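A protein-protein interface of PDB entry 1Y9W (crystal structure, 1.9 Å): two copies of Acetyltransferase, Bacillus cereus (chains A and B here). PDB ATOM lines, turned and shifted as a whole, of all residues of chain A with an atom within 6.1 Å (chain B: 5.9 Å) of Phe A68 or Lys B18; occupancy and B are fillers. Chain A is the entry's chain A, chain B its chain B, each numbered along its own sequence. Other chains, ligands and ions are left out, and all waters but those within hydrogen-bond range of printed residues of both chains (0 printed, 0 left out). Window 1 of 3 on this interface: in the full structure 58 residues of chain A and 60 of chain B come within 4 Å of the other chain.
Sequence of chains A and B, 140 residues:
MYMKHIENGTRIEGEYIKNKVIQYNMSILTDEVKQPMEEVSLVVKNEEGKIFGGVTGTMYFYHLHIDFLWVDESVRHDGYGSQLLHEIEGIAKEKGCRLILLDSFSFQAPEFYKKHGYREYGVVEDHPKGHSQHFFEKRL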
ATOM      1  N   GLY A  54      23.667  30.443  12.630  1.00  0.00           N
ATOM      2  CA  GLY A  54      24.132  29.725  13.803  1.00  0.00           C
ATOM      3  C   GLY A  54      25.109  28.627  13.447  1.00  0.00           C
ATOM      4  O   GLY A  54      25.256  28.265  12.273  1.00  0.00           O
ATOM      5  N   VAL A  55      25.785  28.101  14.461  1.00  0.00           N
ATOM      6  CA  VAL A  55      26.751  27.028  14.267  1.00  0.00           C
ATOM      7  C   VAL A  55      26.746  26.172  15.523  1.00  0.00           C
ATOM      8  O   VAL A  55      26.640  26.693  16.635  1.00  0.00           O
ATOM      9  CB  VAL A  55      28.182  27.592  14.023  1.00  0.00           C
ATOM     10  CG1 VAL A  55      28.643  28.401  15.236  1.00  0.00           C
ATOM     11  CG2 VAL A  55      29.153  26.450  13.715  1.00  0.00           C
ATOM     12  N   THR A  56      26.830  24.860  15.347  1.00  0.00           N
ATOM     13  CA  THR A  56      26.847  23.949  16.484  1.00  0.00           C
ATOM     14  C   THR A  56      27.957  22.932  16.278  1.00  0.00           C
ATOM     15  O   THR A  56      28.277  22.566  15.145  1.00  0.00           O
ATOM     16  CB  THR A  56      25.506  23.182  16.642  1.00  0.00           C
ATOM     17  OG1 THR A  56      25.405  22.176  15.624  1.00  0.00           O
ATOM     18  CG2 THR A  56      24.319  24.141  16.513  1.00  0.00           C
ATOM     19  N   GLY A  57      28.545  22.482  17.379  1.00  0.00           N
ATOM     20  CA  GLY A  57      29.613  21.501  17.305  1.00  0.00           C
ATOM     21  C   GLY A  57      29.724  20.799  18.638  1.00  0.00           C
ATOM     22  O   GLY A  57      29.023  21.163  19.588  1.00  0.00           O
ATOM     23  N   ILE A  66      32.660  20.483  13.969  1.00  0.00           N
ATOM     24  CA  ILE A  66      31.535  21.342  13.634  1.00  0.00           C
ATOM     25  C   ILE A  66      30.464  20.495  12.960  1.00  0.00           C
ATOM     26  O   ILE A  66      30.675  19.951  11.881  1.00  0.00           O
ATOM     27  CB  ILE A  66      31.962  22.492  12.710  1.00  0.00           C
ATOM     28  CG1 ILE A  66      32.993  23.367  13.430  1.00  0.00           C
ATOM     29  CG2 ILE A  66      30.741  23.332  12.327  1.00  0.00           C
ATOM     30  CD1 ILE A  66      33.507  24.509  12.601  1.00  0.00           C
ATOM     31  N   ASP A  67      29.314  20.392  13.620  1.00  0.00           N
ATOM     32  CA  ASP A  67      28.193  19.586  13.145  1.00  0.00           C
ATOM     33  C   ASP A  67      27.316  20.277  12.127  1.00  0.00           C
ATOM     34  O   ASP A  67      26.965  19.701  11.100  1.00  0.00           O
ATOM     35  CB  ASP A  67      27.337  19.162  14.333  1.00  0.00           C
ATOM     36  CG  ASP A  67      28.136  18.429  15.391  1.00  0.00           C
ATOM     37  OD1 ASP A  67      28.881  17.496  15.031  1.00  0.00           O
ATOM     38  OD2 ASP A  67      28.020  18.782  16.582  1.00  0.00           O
ATOM     39  N   PHE A  68      26.940  21.515  12.422  1.00  0.00           N
ATOM     40  CA  PHE A  68      26.093  22.269  11.513  1.00  0.00           C
ATOM     41  C   PHE A  68      26.395  23.761  11.534  1.00  0.00           C
ATOM     42  O   PHE A  68      26.666  24.351  12.584  1.00  0.00           O
ATOM     43  CB  PHE A  68      24.624  22.060  11.878  1.00  0.00           C
ATOM     44  CG  PHE A  68      24.184  20.636  11.800  1.00  0.00           C
ATOM     45  CD1 PHE A  68      23.789  20.086  10.592  1.00  0.00           C
ATOM     46  CD2 PHE A  68      24.194  19.836  12.935  1.00  0.00           C
ATOM     47  CE1 PHE A  68      23.408  18.761  10.507  1.00  0.00           C
ATOM     48  CE2 PHE A  68      23.815  18.508  12.865  1.00  0.00           C
ATOM     49  CZ  PHE A  68      23.421  17.967  11.643  1.00  0.00           C
ATOM     50  N   LEU A  69      26.348  24.362  10.355  1.00  0.00           N
ATOM     51  CA  LEU A  69      26.560  25.793  10.218  1.00  0.00           C
ATOM     52  C   LEU A  69      25.536  26.275   9.205  1.00  0.00           C
ATOM     53  O   LEU A  69      25.494  25.803   8.066  1.00  0.00           O
ATOM     54  CB  LEU A  69      27.975  26.096   9.730  1.00  0.00           C
ATOM     55  CG  LEU A  69      28.314  27.583   9.781  1.00  0.00           C
ATOM     56  CD1 LEU A  69      29.811  27.756   9.839  1.00  0.00           C
ATOM     57  CD2 LEU A  69      27.731  28.284   8.573  1.00  0.00           C
ATOM     58  N   TRP A  70      24.698  27.212   9.625  1.00  0.00           N
ATOM     59  CA  TRP A  70      23.665  27.724   8.745  1.00  0.00           C
ATOM     60  C   TRP A  70      23.517  29.232   8.834  1.00  0.00           C
ATOM     61  O   TRP A  70      23.695  29.831   9.892  1.00  0.00           O
ATOM     62  CB  TRP A  70      22.324  27.068   9.090  1.00  0.00           C
ATOM     63  CG  TRP A  70      21.169  27.616   8.315  1.00  0.00           C
ATOM     64  CD1 TRP A  70      20.823  27.313   7.030  1.00  0.00           C
ATOM     65  CD2 TRP A  70      20.216  28.582   8.771  1.00  0.00           C
ATOM     66  NE1 TRP A  70      19.712  28.028   6.657  1.00  0.00           N
ATOM     67  CE2 TRP A  70      19.319  28.816   7.708  1.00  0.00           C
ATOM     68  CE3 TRP A  70      20.036  29.276   9.974  1.00  0.00           C
ATOM     69  CZ2 TRP A  70      18.253  29.714   7.814  1.00  0.00           C
ATOM     70  CZ3 TRP A  70      18.976  30.170  10.077  1.00  0.00           C
ATOM     71  CH2 TRP A  70      18.101  30.379   9.003  1.00  0.00           C
ATOM     72  N   TYR A 113      34.799  26.604   3.505  1.00  0.00           N
ATOM     73  CA  TYR A 113      35.762  26.134   4.497  1.00  0.00           C
ATOM     74  C   TYR A 113      37.190  26.143   3.967  1.00  0.00           C
ATOM     75  O   TYR A 113      38.135  26.401   4.712  1.00  0.00           O
ATOM     76  CB  TYR A 113      35.375  24.728   4.941  1.00  0.00           C
ATOM     77  CG  TYR A 113      33.982  24.678   5.510  1.00  0.00           C
ATOM     78  CD1 TYR A 113      33.703  25.214   6.763  1.00  0.00           C
ATOM     79  CD2 TYR A 113      32.935  24.126   4.783  1.00  0.00           C
ATOM     80  CE1 TYR A 113      32.412  25.199   7.276  1.00  0.00           C
ATOM     81  CE2 TYR A 113      31.645  24.105   5.284  1.00  0.00           C
ATOM     82  CZ  TYR A 113      31.387  24.640   6.533  1.00  0.00           C
ATOM     83  OH  TYR A 113      30.105  24.587   7.050  1.00  0.00           O
ATOM     84  N   GLU B  13      17.456  26.042  19.950  1.00  0.00           N
ATOM     85  CA  GLU B  13      18.078  26.896  18.954  1.00  0.00           C
ATOM     86  C   GLU B  13      19.050  26.014  18.189  1.00  0.00           C
ATOM     87  O   GLU B  13      19.217  26.157  16.978  1.00  0.00           O
ATOM     88  CB  GLU B  13      18.828  28.045  19.618  1.00  0.00           C
ATOM     89  CG  GLU B  13      17.923  28.975  20.380  1.00  0.00           C
ATOM     90  CD  GLU B  13      18.622  30.240  20.788  1.00  0.00           C
ATOM     91  OE1 GLU B  13      19.647  30.134  21.495  1.00  0.00           O
ATOM     92  OE2 GLU B  13      18.145  31.333  20.399  1.00  0.00           O
ATOM     93  N   GLY B  14      19.681  25.094  18.912  1.00  0.00           N
ATOM     94  CA  GLY B  14      20.621  24.181  18.294  1.00  0.00           C
ATOM     95  C   GLY B  14      19.951  23.255  17.294  1.00  0.00           C
ATOM     96  O   GLY B  14      20.438  23.090  16.174  1.00  0.00           O
ATOM     97  N   GLU B  15      18.833  22.647  17.679  1.00  0.00           N
ATOM     98  CA  GLU B  15      18.151  21.748  16.759  1.00  0.00           C
ATOM     99  C   GLU B  15      17.544  22.535  15.605  1.00  0.00           C
ATOM    100  O   GLU B  15      17.321  21.983  14.526  1.00  0.00           O
ATOM    101  CB  GLU B  15      17.086  20.921  17.479  1.00  0.00           C
ATOM    102  CG  GLU B  15      15.929  21.697  18.018  1.00  0.00           C
ATOM    103  CD  GLU B  15      14.973  20.813  18.803  1.00  0.00           C
ATOM    104  OE1 GLU B  15      15.437  20.136  19.752  1.00  0.00           O
ATOM    105  OE2 GLU B  15      13.763  20.799  18.474  1.00  0.00           O
ATOM    106  N   TYR B  16      17.292  23.822  15.830  1.00  0.00           N
ATOM    107  CA  TYR B  16      16.757  24.681  14.783  1.00  0.00           C
ATOM    108  C   TYR B  16      17.804  24.839  13.663  1.00  0.00           C
ATOM    109  O   TYR B  16      17.472  24.780  12.479  1.00  0.00           O
ATOM    110  CB  TYR B  16      16.411  26.060  15.344  1.00  0.00           C
ATOM    111  CG  TYR B  16      15.862  27.028  14.315  1.00  0.00           C
ATOM    112  CD1 TYR B  16      14.493  27.069  14.022  1.00  0.00           C
ATOM    113  CD2 TYR B  16      16.710  27.906  13.635  1.00  0.00           C
ATOM    114  CE1 TYR B  16      13.986  27.960  13.089  1.00  0.00           C
ATOM    115  CE2 TYR B  16      16.215  28.799  12.694  1.00  0.00           C
ATOM    116  CZ  TYR B  16      14.851  28.825  12.427  1.00  0.00           C
ATOM    117  OH  TYR B  16      14.354  29.729  11.504  1.00  0.00           O
ATOM    118  N   ILE B  17      19.065  25.059  14.026  1.00  0.00           N
ATOM    119  CA  ILE B  17      20.109  25.207  13.011  1.00  0.00           C
ATOM    120  C   ILE B  17      20.229  23.901  12.224  1.00  0.00           C
ATOM    121  O   ILE B  17      20.319  23.908  10.996  1.00  0.00           O
ATOM    122  CB  ILE B  17      21.487  25.543  13.652  1.00  0.00           C
ATOM    123  CG1 ILE B  17      21.407  26.876  14.409  1.00  0.00           C
ATOM    124  CG2 ILE B  17      22.567  25.602  12.571  1.00  0.00           C
ATOM    125  CD1 ILE B  17      21.117  28.078  13.517  1.00  0.00           C
ATOM    126  N   LYS B  18      20.218  22.780  12.944  1.00  0.00           N
ATOM    127  CA  LYS B  18      20.316  21.468  12.321  1.00  0.00           C
ATOM    128  C   LYS B  18      19.182  21.230  11.332  1.00  0.00           C
ATOM    129  O   LYS B  18      19.415  20.794  10.211  1.00  0.00           O
ATOM    130  CB  LYS B  18      20.302  20.373  13.386  1.00  0.00           C
ATOM    131  CG  LYS B  18      20.146  18.989  12.788  1.00  0.00           C
ATOM    132  CD  LYS B  18      20.246  17.884  13.799  1.00  0.00           C
ATOM    133  CE  LYS B  18      20.178  16.550  13.082  1.00  0.00           C
ATOM    134  NZ  LYS B  18      20.471  15.403  13.982  1.00  0.00           N
ATOM    135  N   ASN B  19      17.955  21.509  11.764  1.00  0.00           N
ATOM    136  CA  ASN B  19      16.770  21.344  10.927  1.00  0.00           C
ATOM    137  C   ASN B  19      16.832  22.186   9.672  1.00  0.00           C
ATOM    138  O   ASN B  19      16.345  21.772   8.623  1.00  0.00           O
ATOM    139  CB  ASN B  19      15.513  21.712  11.707  1.00  0.00           C
ATOM    140  CG  ASN B  19      14.931  20.537  12.448  1.00  0.00           C
ATOM    141  OD1 ASN B  19      15.661  19.687  12.964  1.00  0.00           O
ATOM    142  ND2 ASN B  19      13.607  20.477  12.510  1.00  0.00           N
ATOM    143  N   LYS B  20      17.413  23.376   9.785  1.00  0.00           N
ATOM    144  CA  LYS B  20      17.549  24.271   8.637  1.00  0.00           C
ATOM    145  C   LYS B  20      18.529  23.700   7.613  1.00  0.00           C
ATOM    146  O   LYS B  20      18.311  23.808   6.411  1.00  0.00           O
ATOM    147  CB  LYS B  20      18.024  25.657   9.095  1.00  0.00           C
ATOM    148  CG  LYS B  20      16.905  26.554   9.621  1.00  0.00           C
ATOM    149  CD  LYS B  20      15.913  26.877   8.509  1.00  0.00           C
ATOM    150  CE  LYS B  20      14.796  27.795   8.969  1.00  0.00           C
ATOM    151  NZ  LYS B  20      13.844  28.070   7.855  1.00  0.00           N
ATOM    152  N   VAL B  21      19.613  23.097   8.091  1.00  0.00           N
ATOM    153  CA  VAL B  21      20.605  22.506   7.200  1.00  0.00           C
ATOM    154  C   VAL B  21      19.989  21.289   6.516  1.00  0.00           C
ATOM    155  O   VAL B  21      20.120  21.102   5.310  1.00  0.00           O
ATOM    156  CB  VAL B  21      21.865  22.080   7.983  1.00  0.00           C
ATOM    157  CG1 VAL B  21      22.806  21.290   7.086  1.00  0.00           C
ATOM    158  CG2 VAL B  21      22.573  23.303   8.518  1.00  0.00           C
ATOM    159  N   ILE B  22      19.305  20.462   7.289  1.00  0.00           N
ATOM    160  CA  ILE B  22      18.675  19.284   6.729  1.00  0.00           C
ATOM    161  C   ILE B  22      17.656  19.706   5.686  1.00  0.00           C
ATOM    162  O   ILE B  22      17.530  19.082   4.631  1.00  0.00           O
ATOM    163  CB  ILE B  22      17.985  18.477   7.823  1.00  0.00           C
ATOM    164  CG1 ILE B  22      19.049  17.804   8.693  1.00  0.00           C
ATOM    165  CG2 ILE B  22      17.020  17.472   7.204  1.00  0.00           C
ATOM    166  CD1 ILE B  22      18.482  17.110   9.918  1.00  0.00           C
ATOM    167  N   GLN B  23      16.937  20.777   5.990  1.00  0.00           N
ATOM    168  CA  GLN B  23      15.922  21.306   5.094  1.00  0.00           C
ATOM    169  C   GLN B  23      16.541  21.740   3.759  1.00  0.00           C
ATOM    170  O   GLN B  23      16.027  21.420   2.682  1.00  0.00           O
ATOM    171  CB  GLN B  23      15.246  22.486   5.769  1.00  0.00           C
ATOM    172  CG  GLN B  23      13.941  22.894   5.159  1.00  0.00           C
ATOM    173  CD  GLN B  23      13.327  24.059   5.907  1.00  0.00           C
ATOM    174  OE1 GLN B  23      13.785  25.202   5.790  1.00  0.00           O
ATOM    175  NE2 GLN B  23      12.296  23.772   6.700  1.00  0.00           N
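N of Thr A56 sits at hydrogen-bond distance from O of Phe A68, at 2.8 Å. The backbone carbonyl oxygen (O) of Trp A70 sits at hydrogen-bond distance from the backbone NH (N) of Gly A54 (2.8 Å).
Among the printed residues, merely in contact across the chains: Gly A54 with Ile B17 (3.4 Å), Phe A68 with Lys B18 (3.6 Å), Phe A68 with Val B21 (3.8 Å), Leu A69 with Val B21 (3.9 Å), Trp A70 with Ile B17 (3.8 Å), Trp A70 with Lys B20 (3.7 Å) and Trp A70 with Val B21 (3.8 Å).
Phe A68 touches just these residues of chain B: Lys B18 (3.6 Å) and Val B21 (3.8 Å). Lys B18 touches just one residue of chain A: Phe A68. Of the printed residues of chain B, Leu A69 touches Val B21 (3.9 Å). Printed residues of chain B within 4 Å of Gly A54: Ile B17 (3.4 Å). Printed residues of chain A within 4 Å of Val B21: Phe A68 (3.8 Å), Leu A69 (3.9 Å) and Trp A70 (3.8 Å). Of the printed residues of chain B, Trp A70 touches Ile B17 (3.8 Å), Lys B20 (3.7 Å) and Val B21 (3.8 Å). Of the printed residues of chain A, Lys B20 touches Trp A70. Tyr A113 touches none of the printed residues of chain B. Glu B15 touches none of the printed residues of chain A. The nearest residue of chain B that does not touch Phe A68 is Ile B17 (4.2 Å). The nearest residue of chain A that does not touch Lys B18 is Thr A56 (5.6 Å). The nearest printed residue of chain A that does not touch Lys B20 is Phe A68 (7.0 Å).
Hydrophobic or aromatic side chains of chain A that line the printed part of chain B: Phe A68 and Trp A70. Among the printed residues, 7 pairs touch across the chains.
No position is printed for both chains. Of the 7 pairs that touch across the chains among the printed residues, none has its exchanged pair printed and touching as well.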
